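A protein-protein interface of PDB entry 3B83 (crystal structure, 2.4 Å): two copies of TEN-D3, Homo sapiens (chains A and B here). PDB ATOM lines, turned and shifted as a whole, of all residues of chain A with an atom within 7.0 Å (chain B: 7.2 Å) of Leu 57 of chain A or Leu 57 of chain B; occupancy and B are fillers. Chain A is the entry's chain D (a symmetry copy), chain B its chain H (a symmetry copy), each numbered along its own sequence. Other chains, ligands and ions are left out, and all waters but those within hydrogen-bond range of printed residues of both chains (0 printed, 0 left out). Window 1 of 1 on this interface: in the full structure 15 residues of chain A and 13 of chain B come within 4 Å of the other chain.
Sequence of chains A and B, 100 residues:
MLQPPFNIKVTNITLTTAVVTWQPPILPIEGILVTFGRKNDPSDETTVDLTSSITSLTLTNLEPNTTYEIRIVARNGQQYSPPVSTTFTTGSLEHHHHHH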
ATOM      1  N   ALA A  18     -18.811 -29.625 -22.545  1.00  0.00           N
ATOM      2  CA  ALA A  18     -18.832 -29.882 -21.122  1.00  0.00           C
ATOM      3  C   ALA A  18     -19.149 -28.585 -20.387  1.00  0.00           C
ATOM      4  O   ALA A  18     -18.803 -27.505 -20.860  1.00  0.00           O
ATOM      5  CB  ALA A  18     -17.475 -30.429 -20.670  1.00  0.00           C
ATOM      6  N   VAL A  19     -19.798 -28.705 -19.230  1.00  0.00           N
ATOM      7  CA  VAL A  19     -20.162 -27.563 -18.402  1.00  0.00           C
ATOM      8  C   VAL A  19     -19.289 -27.509 -17.141  1.00  0.00           C
ATOM      9  O   VAL A  19     -19.243 -28.463 -16.361  1.00  0.00           O
ATOM     10  CB  VAL A  19     -21.648 -27.654 -17.947  1.00  0.00           C
ATOM     11  CG1 VAL A  19     -21.941 -26.598 -16.884  1.00  0.00           C
ATOM     12  CG2 VAL A  19     -22.572 -27.485 -19.138  1.00  0.00           C
ATOM     13  N   VAL A  20     -18.613 -26.386 -16.927  1.00  0.00           N
ATOM     14  CA  VAL A  20     -17.775 -26.225 -15.745  1.00  0.00           C
ATOM     15  C   VAL A  20     -18.412 -25.253 -14.763  1.00  0.00           C
ATOM     16  O   VAL A  20     -18.782 -24.153 -15.141  1.00  0.00           O
ATOM     17  CB  VAL A  20     -16.395 -25.663 -16.115  1.00  0.00           C
ATOM     18  CG1 VAL A  20     -15.478 -25.726 -14.919  1.00  0.00           C
ATOM     19  CG2 VAL A  20     -15.821 -26.423 -17.292  1.00  0.00           C
ATOM     20  N   THR A  21     -18.543 -25.652 -13.506  1.00  0.00           N
ATOM     21  CA  THR A  21     -19.110 -24.774 -12.485  1.00  0.00           C
ATOM     22  C   THR A  21     -18.166 -24.707 -11.266  1.00  0.00           C
ATOM     23  O   THR A  21     -17.384 -25.632 -11.017  1.00  0.00           O
ATOM     24  CB  THR A  21     -20.527 -25.254 -12.034  1.00  0.00           C
ATOM     25  OG1 THR A  21     -20.515 -26.671 -11.827  1.00  0.00           O
ATOM     26  CG2 THR A  21     -21.583 -24.921 -13.086  1.00  0.00           C
ATOM     27  N   TRP A  22     -18.227 -23.611 -10.515  1.00  0.00           N
ATOM     28  CA  TRP A  22     -17.366 -23.450  -9.348  1.00  0.00           C
ATOM     29  C   TRP A  22     -17.924 -22.420  -8.374  1.00  0.00           C
ATOM     30  O   TRP A  22     -18.889 -21.719  -8.679  1.00  0.00           O
ATOM     31  CB  TRP A  22     -15.960 -23.037  -9.797  1.00  0.00           C
ATOM     32  CG  TRP A  22     -15.907 -21.683 -10.434  1.00  0.00           C
ATOM     33  CD1 TRP A  22     -15.727 -20.485  -9.803  1.00  0.00           C
ATOM     34  CD2 TRP A  22     -16.086 -21.378 -11.826  1.00  0.00           C
ATOM     35  NE1 TRP A  22     -15.782 -19.456 -10.712  1.00  0.00           N
ATOM     36  CE2 TRP A  22     -16.002 -19.975 -11.960  1.00  0.00           C
ATOM     37  CE3 TRP A  22     -16.312 -22.154 -12.971  1.00  0.00           C
ATOM     38  CZ2 TRP A  22     -16.138 -19.331 -13.193  1.00  0.00           C
ATOM     39  CZ3 TRP A  22     -16.446 -21.508 -14.199  1.00  0.00           C
ATOM     40  CH2 TRP A  22     -16.357 -20.112 -14.298  1.00  0.00           C
ATOM     41  N   VAL A  34      -9.368 -18.945 -15.547  1.00  0.00           N
ATOM     42  CA  VAL A  34      -9.762 -20.314 -15.814  1.00  0.00           C
ATOM     43  C   VAL A  34      -8.931 -20.827 -16.985  1.00  0.00           C
ATOM     44  O   VAL A  34      -8.891 -20.208 -18.042  1.00  0.00           O
ATOM     45  CB  VAL A  34     -11.270 -20.389 -16.137  1.00  0.00           C
ATOM     46  CG1 VAL A  34     -11.750 -21.833 -16.122  1.00  0.00           C
ATOM     47  CG2 VAL A  34     -12.046 -19.574 -15.114  1.00  0.00           C
ATOM     48  N   PHE A  36      -7.799 -24.396 -19.319  1.00  0.00           N
ATOM     49  CA  PHE A  36      -8.237 -25.725 -19.713  1.00  0.00           C
ATOM     50  C   PHE A  36      -7.471 -26.254 -20.927  1.00  0.00           C
ATOM     51  O   PHE A  36      -6.953 -25.484 -21.744  1.00  0.00           O
ATOM     52  CB  PHE A  36      -9.752 -25.716 -20.000  1.00  0.00           C
ATOM     53  CG  PHE A  36     -10.172 -24.733 -21.071  1.00  0.00           C
ATOM     54  CD1 PHE A  36     -10.527 -25.174 -22.341  1.00  0.00           C
ATOM     55  CD2 PHE A  36     -10.213 -23.362 -20.806  1.00  0.00           C
ATOM     56  CE1 PHE A  36     -10.918 -24.268 -23.339  1.00  0.00           C
ATOM     57  CE2 PHE A  36     -10.602 -22.447 -21.797  1.00  0.00           C
ATOM     58  CZ  PHE A  36     -10.955 -22.906 -23.065  1.00  0.00           C
ATOM     59  N   VAL A  48      -8.806 -17.834 -19.879  1.00  0.00           N
ATOM     60  CA  VAL A  48      -9.740 -16.713 -19.905  1.00  0.00           C
ATOM     61  C   VAL A  48      -9.768 -15.998 -18.549  1.00  0.00           C
ATOM     62  O   VAL A  48      -9.663 -16.643 -17.501  1.00  0.00           O
ATOM     63  CB  VAL A  48     -11.173 -17.198 -20.205  1.00  0.00           C
ATOM     64  CG1 VAL A  48     -12.073 -16.012 -20.380  1.00  0.00           C
ATOM     65  CG2 VAL A  48     -11.198 -18.051 -21.445  1.00  0.00           C
ATOM     66  N   LEU A  50     -12.042 -13.974 -15.980  1.00  0.00           N
ATOM     67  CA  LEU A  50     -13.434 -13.644 -15.656  1.00  0.00           C
ATOM     68  C   LEU A  50     -13.582 -12.774 -14.422  1.00  0.00           C
ATOM     69  O   LEU A  50     -12.601 -12.483 -13.756  1.00  0.00           O
ATOM     70  CB  LEU A  50     -14.234 -14.934 -15.441  1.00  0.00           C
ATOM     71  CG  LEU A  50     -14.017 -16.024 -16.499  1.00  0.00           C
ATOM     72  CD1 LEU A  50     -14.844 -17.243 -16.140  1.00  0.00           C
ATOM     73  CD2 LEU A  50     -14.384 -15.503 -17.878  1.00  0.00           C
ATOM     74  N   ILE A  54     -19.057 -14.473 -12.184  1.00  0.00           N
ATOM     75  CA  ILE A  54     -19.423 -15.518 -13.136  1.00  0.00           C
ATOM     76  C   ILE A  54     -19.083 -16.853 -12.477  1.00  0.00           C
ATOM     77  O   ILE A  54     -17.988 -17.016 -11.929  1.00  0.00           O
ATOM     78  CB  ILE A  54     -18.671 -15.344 -14.473  1.00  0.00           C
ATOM     79  CG1 ILE A  54     -19.110 -14.033 -15.134  1.00  0.00           C
ATOM     80  CG2 ILE A  54     -18.947 -16.525 -15.391  1.00  0.00           C
ATOM     81  CD1 ILE A  54     -18.307 -13.646 -16.326  1.00  0.00           C
ATOM     82  N   THR A  55     -20.017 -17.800 -12.523  1.00  0.00           N
ATOM     83  CA  THR A  55     -19.803 -19.070 -11.865  1.00  0.00           C
ATOM     84  C   THR A  55     -19.850 -20.328 -12.708  1.00  0.00           C
ATOM     85  O   THR A  55     -19.839 -21.428 -12.166  1.00  0.00           O
ATOM     86  CB  THR A  55     -20.770 -19.230 -10.697  1.00  0.00           C
ATOM     87  OG1 THR A  55     -22.108 -19.366 -11.185  1.00  0.00           O
ATOM     88  CG2 THR A  55     -20.687 -18.009  -9.795  1.00  0.00           C
ATOM     89  N   SER A  56     -19.897 -20.183 -14.024  1.00  0.00           N
ATOM     90  CA  SER A  56     -19.875 -21.352 -14.893  1.00  0.00           C
ATOM     91  C   SER A  56     -19.660 -21.020 -16.351  1.00  0.00           C
ATOM     92  O   SER A  56     -20.006 -19.940 -16.827  1.00  0.00           O
ATOM     93  CB  SER A  56     -21.146 -22.182 -14.752  1.00  0.00           C
ATOM     94  OG  SER A  56     -22.277 -21.363 -14.904  1.00  0.00           O
ATOM     95  N   LEU A  57     -19.078 -21.987 -17.044  1.00  0.00           N
ATOM     96  CA  LEU A  57     -18.762 -21.893 -18.453  1.00  0.00           C
ATOM     97  C   LEU A  57     -19.214 -23.179 -19.104  1.00  0.00           C
ATOM     98  O   LEU A  57     -19.311 -24.213 -18.440  1.00  0.00           O
ATOM     99  CB  LEU A  57     -17.252 -21.814 -18.655  1.00  0.00           C
ATOM    100  CG  LEU A  57     -16.471 -20.517 -18.613  1.00  0.00           C
ATOM    101  CD1 LEU A  57     -17.258 -19.448 -17.916  1.00  0.00           C
ATOM    102  CD2 LEU A  57     -15.141 -20.789 -17.930  1.00  0.00           C
ATOM    103  N   THR A  58     -19.468 -23.106 -20.404  1.00  0.00           N
ATOM    104  CA  THR A  58     -19.822 -24.276 -21.179  1.00  0.00           C
ATOM    105  C   THR A  58     -18.727 -24.290 -22.244  1.00  0.00           C
ATOM    106  O   THR A  58     -18.456 -23.271 -22.878  1.00  0.00           O
ATOM    107  CB  THR A  58     -21.212 -24.136 -21.808  1.00  0.00           C
ATOM    108  OG1 THR A  58     -22.190 -24.035 -20.766  1.00  0.00           O
ATOM    109  CG2 THR A  58     -21.538 -25.352 -22.665  1.00  0.00           C
ATOM    110  N   LEU A  59     -18.068 -25.430 -22.412  1.00  0.00           N
ATOM    111  CA  LEU A  59     -16.983 -25.550 -23.379  1.00  0.00           C
ATOM    112  C   LEU A  59     -17.365 -26.380 -24.597  1.00  0.00           C
ATOM    113  O   LEU A  59     -18.062 -27.389 -24.479  1.00  0.00           O
ATOM    114  CB  LEU A  59     -15.767 -26.176 -22.705  1.00  0.00           C
ATOM    115  CG  LEU A  59     -15.164 -25.385 -21.541  1.00  0.00           C
ATOM    116  CD1 LEU A  59     -14.119 -26.236 -20.838  1.00  0.00           C
ATOM    117  CD2 LEU A  59     -14.545 -24.084 -22.055  1.00  0.00           C
ATOM    118  N   ILE A  72      -8.507 -23.222 -11.896  1.00  0.00           N
ATOM    119  CA  ILE A  72      -9.125 -21.926 -11.646  1.00  0.00           C
ATOM    120  C   ILE A  72      -8.300 -21.236 -10.573  1.00  0.00           C
ATOM    121  O   ILE A  72      -8.082 -21.779  -9.490  1.00  0.00           O
ATOM    122  CB  ILE A  72     -10.571 -22.049 -11.145  1.00  0.00           C
ATOM    123  CG1 ILE A  72     -11.447 -22.660 -12.225  1.00  0.00           C
ATOM    124  CG2 ILE A  72     -11.112 -20.680 -10.787  1.00  0.00           C
ATOM    125  CD1 ILE A  72     -12.872 -22.862 -11.771  1.00  0.00           C
ATOM    126  N   LYS B   9     -29.460 -16.341 -26.244  1.00  0.00           N
ATOM    127  CA  LYS B   9     -30.572 -16.719 -25.381  1.00  0.00           C
ATOM    128  C   LYS B   9     -30.209 -16.556 -23.918  1.00  0.00           C
ATOM    129  O   LYS B   9     -29.074 -16.817 -23.523  1.00  0.00           O
ATOM    130  CB  LYS B   9     -30.961 -18.177 -25.619  1.00  0.00           C
ATOM    131  CG  LYS B   9     -31.719 -18.434 -26.906  1.00  0.00           C
ATOM    132  CD  LYS B   9     -32.278 -19.857 -26.915  1.00  0.00           C
ATOM    133  CE  LYS B   9     -33.142 -20.132 -28.144  1.00  0.00           C
ATOM    134  NZ  LYS B   9     -33.825 -21.464 -28.049  1.00  0.00           N
ATOM    135  N   ALA B  18     -28.623 -15.407 -14.069  1.00  0.00           N
ATOM    136  CA  ALA B  18     -29.120 -15.611 -15.417  1.00  0.00           C
ATOM    137  C   ALA B  18     -28.083 -16.410 -16.196  1.00  0.00           C
ATOM    138  O   ALA B  18     -26.884 -16.277 -15.961  1.00  0.00           O
ATOM    139  CB  ALA B  18     -29.374 -14.265 -16.094  1.00  0.00           C
ATOM    140  N   VAL B  19     -28.543 -17.258 -17.102  1.00  0.00           N
ATOM    141  CA  VAL B  19     -27.642 -18.042 -17.918  1.00  0.00           C
ATOM    142  C   VAL B  19     -27.694 -17.467 -19.328  1.00  0.00           C
ATOM    143  O   VAL B  19     -28.773 -17.244 -19.872  1.00  0.00           O
ATOM    144  CB  VAL B  19     -28.062 -19.529 -17.967  1.00  0.00           C
ATOM    145  CG1 VAL B  19     -27.311 -20.235 -19.083  1.00  0.00           C
ATOM    146  CG2 VAL B  19     -27.752 -20.222 -16.637  1.00  0.00           C
ATOM    147  N   VAL B  20     -26.533 -17.204 -19.913  1.00  0.00           N
ATOM    148  CA  VAL B  20     -26.466 -16.679 -21.266  1.00  0.00           C
ATOM    149  C   VAL B  20     -25.828 -17.721 -22.180  1.00  0.00           C
ATOM    150  O   VAL B  20     -24.825 -18.339 -21.822  1.00  0.00           O
ATOM    151  CB  VAL B  20     -25.603 -15.415 -21.339  1.00  0.00           C
ATOM    152  CG1 VAL B  20     -25.823 -14.718 -22.671  1.00  0.00           C
ATOM    153  CG2 VAL B  20     -25.929 -14.510 -20.193  1.00  0.00           C
ATOM    154  N   THR B  21     -26.399 -17.895 -23.367  1.00  0.00           N
ATOM    155  CA  THR B  21     -25.889 -18.852 -24.343  1.00  0.00           C
ATOM    156  C   THR B  21     -25.967 -18.226 -25.737  1.00  0.00           C
ATOM    157  O   THR B  21     -26.817 -17.366 -25.993  1.00  0.00           O
ATOM    158  CB  THR B  21     -26.722 -20.148 -24.328  1.00  0.00           C
ATOM    159  OG1 THR B  21     -26.784 -20.650 -22.995  1.00  0.00           O
ATOM    160  CG2 THR B  21     -26.100 -21.205 -25.206  1.00  0.00           C
ATOM    161  N   TRP B  22     -25.087 -18.654 -26.636  1.00  0.00           N
ATOM    162  CA  TRP B  22     -25.062 -18.122 -27.992  1.00  0.00           C
ATOM    163  C   TRP B  22     -24.276 -19.104 -28.859  1.00  0.00           C
ATOM    164  O   TRP B  22     -23.780 -20.113 -28.358  1.00  0.00           O
ATOM    165  CB  TRP B  22     -24.371 -16.753 -27.978  1.00  0.00           C
ATOM    166  CG  TRP B  22     -22.901 -16.853 -27.630  1.00  0.00           C
ATOM    167  CD1 TRP B  22     -21.872 -17.092 -28.494  1.00  0.00           C
ATOM    168  CD2 TRP B  22     -22.319 -16.831 -26.315  1.00  0.00           C
ATOM    169  NE1 TRP B  22     -20.691 -17.229 -27.804  1.00  0.00           N
ATOM    170  CE2 TRP B  22     -20.936 -17.071 -26.465  1.00  0.00           C
ATOM    171  CE3 TRP B  22     -22.836 -16.635 -25.027  1.00  0.00           C
ATOM    172  CZ2 TRP B  22     -20.057 -17.122 -25.376  1.00  0.00           C
ATOM    173  CZ3 TRP B  22     -21.959 -16.684 -23.942  1.00  0.00           C
ATOM    174  CH2 TRP B  22     -20.585 -16.926 -24.127  1.00  0.00           C
ATOM    175  N   VAL B  34     -18.060 -10.485 -24.457  1.00  0.00           N
ATOM    176  CA  VAL B  34     -19.397 -10.478 -23.884  1.00  0.00           C
ATOM    177  C   VAL B  34     -19.475  -9.292 -22.938  1.00  0.00           C
ATOM    178  O   VAL B  34     -18.713  -9.203 -21.974  1.00  0.00           O
ATOM    179  CB  VAL B  34     -19.689 -11.785 -23.114  1.00  0.00           C
ATOM    180  CG1 VAL B  34     -21.142 -11.809 -22.650  1.00  0.00           C
ATOM    181  CG2 VAL B  34     -19.395 -12.975 -24.004  1.00  0.00           C
ATOM    182  N   PHE B  36     -21.967  -7.056 -20.446  1.00  0.00           N
ATOM    183  CA  PHE B  36     -23.229  -7.075 -19.721  1.00  0.00           C
ATOM    184  C   PHE B  36     -23.281  -5.997 -18.644  1.00  0.00           C
ATOM    185  O   PHE B  36     -22.245  -5.494 -18.204  1.00  0.00           O
ATOM    186  CB  PHE B  36     -23.460  -8.462 -19.109  1.00  0.00           C
ATOM    187  CG  PHE B  36     -22.372  -8.908 -18.179  1.00  0.00           C
ATOM    188  CD1 PHE B  36     -22.373  -8.516 -16.846  1.00  0.00           C
ATOM    189  CD2 PHE B  36     -21.339  -9.719 -18.638  1.00  0.00           C
ATOM    190  CE1 PHE B  36     -21.358  -8.927 -15.976  1.00  0.00           C
ATOM    191  CE2 PHE B  36     -20.316 -10.137 -17.776  1.00  0.00           C
ATOM    192  CZ  PHE B  36     -20.328  -9.739 -16.442  1.00  0.00           C
ATOM    193  N   VAL B  48     -15.978  -9.123 -20.954  1.00  0.00           N
ATOM    194  CA  VAL B  48     -15.126 -10.282 -20.771  1.00  0.00           C
ATOM    195  C   VAL B  48     -14.631 -10.781 -22.128  1.00  0.00           C
ATOM    196  O   VAL B  48     -15.405 -10.887 -23.072  1.00  0.00           O
ATOM    197  CB  VAL B  48     -15.885 -11.401 -20.029  1.00  0.00           C
ATOM    198  CG1 VAL B  48     -15.077 -12.683 -20.048  1.00  0.00           C
ATOM    199  CG2 VAL B  48     -16.132 -10.989 -18.586  1.00  0.00           C
ATOM    200  N   LEU B  50     -13.344 -13.752 -24.282  1.00  0.00           N
ATOM    201  CA  LEU B  50     -13.349 -15.210 -24.272  1.00  0.00           C
ATOM    202  C   LEU B  50     -12.811 -15.864 -25.523  1.00  0.00           C
ATOM    203  O   LEU B  50     -12.607 -15.218 -26.545  1.00  0.00           O
ATOM    204  CB  LEU B  50     -14.772 -15.733 -24.082  1.00  0.00           C
ATOM    205  CG  LEU B  50     -15.663 -15.221 -22.957  1.00  0.00           C
ATOM    206  CD1 LEU B  50     -17.047 -15.793 -23.144  1.00  0.00           C
ATOM    207  CD2 LEU B  50     -15.102 -15.638 -21.616  1.00  0.00           C
ATOM    208  N   ILE B  54     -16.036 -21.156 -26.121  1.00  0.00           N
ATOM    209  CA  ILE B  54     -16.935 -21.084 -24.969  1.00  0.00           C
ATOM    210  C   ILE B  54     -18.273 -20.560 -25.489  1.00  0.00           C
ATOM    211  O   ILE B  54     -18.307 -19.645 -26.309  1.00  0.00           O
ATOM    212  CB  ILE B  54     -16.391 -20.145 -23.873  1.00  0.00           C
ATOM    213  CG1 ILE B  54     -15.216 -20.824 -23.154  1.00  0.00           C
ATOM    214  CG2 ILE B  54     -17.512 -19.783 -22.904  1.00  0.00           C
ATOM    215  CD1 ILE B  54     -14.608 -20.016 -22.032  1.00  0.00           C
ATOM    216  N   THR B  55     -19.376 -21.131 -25.028  1.00  0.00           N
ATOM    217  CA  THR B  55     -20.677 -20.704 -25.529  1.00  0.00           C
ATOM    218  C   THR B  55     -21.704 -20.342 -24.469  1.00  0.00           C
ATOM    219  O   THR B  55     -22.867 -20.137 -24.798  1.00  0.00           O
ATOM    220  CB  THR B  55     -21.320 -21.798 -26.405  1.00  0.00           C
ATOM    221  OG1 THR B  55     -21.468 -22.985 -25.622  1.00  0.00           O
ATOM    222  CG2 THR B  55     -20.475 -22.104 -27.618  1.00  0.00           C
ATOM    223  N   SER B  56     -21.303 -20.260 -23.207  1.00  0.00           N
ATOM    224  CA  SER B  56     -22.273 -19.945 -22.168  1.00  0.00           C
ATOM    225  C   SER B  56     -21.629 -19.495 -20.862  1.00  0.00           C
ATOM    226  O   SER B  56     -20.559 -19.969 -20.489  1.00  0.00           O
ATOM    227  CB  SER B  56     -23.157 -21.174 -21.917  1.00  0.00           C
ATOM    228  OG  SER B  56     -24.212 -20.913 -21.008  1.00  0.00           O
ATOM    229  N   LEU B  57     -22.297 -18.577 -20.175  1.00  0.00           N
ATOM    230  CA  LEU B  57     -21.835 -18.068 -18.899  1.00  0.00           C
ATOM    231  C   LEU B  57     -23.037 -17.995 -17.991  1.00  0.00           C
ATOM    232  O   LEU B  57     -24.160 -17.842 -18.458  1.00  0.00           O
ATOM    233  CB  LEU B  57     -21.292 -16.647 -19.024  1.00  0.00           C
ATOM    234  CG  LEU B  57     -20.104 -16.382 -19.925  1.00  0.00           C
ATOM    235  CD1 LEU B  57     -19.800 -14.880 -19.946  1.00  0.00           C
ATOM    236  CD2 LEU B  57     -18.915 -17.186 -19.420  1.00  0.00           C
ATOM    237  N   THR B  58     -22.802 -18.095 -16.692  1.00  0.00           N
ATOM    238  CA  THR B  58     -23.872 -17.966 -15.736  1.00  0.00           C
ATOM    239  C   THR B  58     -23.460 -16.752 -14.916  1.00  0.00           C
ATOM    240  O   THR B  58     -22.371 -16.712 -14.373  1.00  0.00           O
ATOM    241  CB  THR B  58     -23.992 -19.205 -14.839  1.00  0.00           C
ATOM    242  OG1 THR B  58     -24.417 -20.329 -15.618  1.00  0.00           O
ATOM    243  CG2 THR B  58     -24.997 -18.962 -13.742  1.00  0.00           C
ATOM    244  N   LEU B  59     -24.318 -15.745 -14.865  1.00  0.00           N
ATOM    245  CA  LEU B  59     -24.018 -14.533 -14.116  1.00  0.00           C
ATOM    246  C   LEU B  59     -24.689 -14.604 -12.756  1.00  0.00           C
ATOM    247  O   LEU B  59     -25.803 -15.103 -12.633  1.00  0.00           O
ATOM    248  CB  LEU B  59     -24.528 -13.306 -14.875  1.00  0.00           C
ATOM    249  CG  LEU B  59     -24.075 -13.166 -16.329  1.00  0.00           C
ATOM    250  CD1 LEU B  59     -24.792 -11.998 -16.983  1.00  0.00           C
ATOM    251  CD2 LEU B  59     -22.586 -12.957 -16.382  1.00  0.00           C
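N of Thr 55 of chain A lies within hydrogen-bond range of O of Thr 58 of chain B (3.2 Å). The backbone NH (N) of Thr 55 of chain B is in hydrogen-bond range of the backbone carbonyl oxygen (O) of Thr 58 of chain A (3.2 Å). N of Thr 58 of chain A sits at hydrogen-bond distance from O of Ser 56 of chain B. OG of Ser 56 of chain A lies within hydrogen-bond range of OG1 of Thr 58 of chain B (2.5 Å).
Ile 54 of chain A touches Leu 59 of chain B, and with the chains exchanged Leu 59 of chain A touches Ile 54 of chain B. Ser 56 of chain A touches its own counterpart, Ser 56 of chain B. Ser 56 of chain A touches Thr 58 of chain B, and with the chains exchanged Thr 58 of chain A touches Ser 56 of chain B. Leu 57 of chain A touches Ile 54 of chain B, but with the chains exchanged Ile 54 of chain A does not touch Leu 57 of chain B (4.1 Å). 15 positions are printed for both chains. Of the 17 pairs that touch across the chains among the printed residues, 15 have their exchanged pair printed and touching as well.
O of Val 34 of chain B is in hydrogen-bond range of N of Val 48 of chain B (2.9 Å). N of Val 20 of chain B sits at hydrogen-bond distance from O of Leu 57 of chain B (2.9 Å). The side-chain hydroxyl (OG1) of Thr 21 of chain B is in hydrogen-bond range of the side-chain hydroxyl (OG) of Ser 56 of chain B (3.3 Å). The backbone carbonyl oxygen of Ala 18 of chain A sits at hydrogen-bond distance from the backbone NH of Leu 59 of chain A. The backbone carbonyl oxygen (O) of Leu 57 of chain A sits at hydrogen-bond distance from the backbone NH (N) of Val 20 of chain A (2.7 Å). The backbone NH of Val 48 of chain A lies within hydrogen-bond range of the backbone carbonyl oxygen of Val 34 of chain A.
Val 20 of chain A touches none of the printed residues of chain B. Printed residues of chain B within 4 Å of Ser 56 of chain A: Ser 56 (3.7 Å), Leu 57 (3.3 Å) and Thr 58 (2.5 Å). Leu 57 of chain A touches just these residues of chain B: Ile 54, Ser 56 and Leu 57. Lys 9 of chain B touches none of the printed residues of chain A. Of the printed residues of chain A, Thr 55 of chain B touches Thr 58 (3.2 Å). Of the printed residues of chain A, Ser 56 of chain B touches Ser 56, Leu 57 and Thr 58. The nearest printed residue of chain A that does not touch Ser 56 of chain B is Leu 59 of chain A (6.2 Å).
Hydrophobic or aromatic side chains of chain B within 4 Å of the printed part of chain A: Val 48, Leu 50, Ile 54, Leu 57 and Leu 59. Of the 16 printed residues of chain A, 8 touch a printed residue of chain B. Among the printed residues, 17 pairs touch across the chains.
Leu 50 of chain B touches Val 48 of chain A. Ile 54 of chain B touches Val 48 of chain A (CD1 to CG2, 3.98 Å). Val 48 of chain B touches Leu 50 of chain A (CG1 to CD2, 3.6 Å). Leu 50 of chain A touches Leu 50 of chain B. Ser 56 of chain A touches Ser 56 of chain B (O to O, 3.7 Å). Leu 57 of chain A touches Ile 54 of chain B (CG to CD1, 3.9 Å). Ser 56 of chain B touches Leu 57 of chain A. CD1 of Leu 57 of chain A touches CD2 of Leu 57 of chain B, 3.2 Å away. O of Thr 58 of chain A touches CA of Ile 54 of chain B, 3.4 Å away. CD2 of Leu 59 of chain A touches CG1 of Ile 54 of chain B (3.5 Å).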
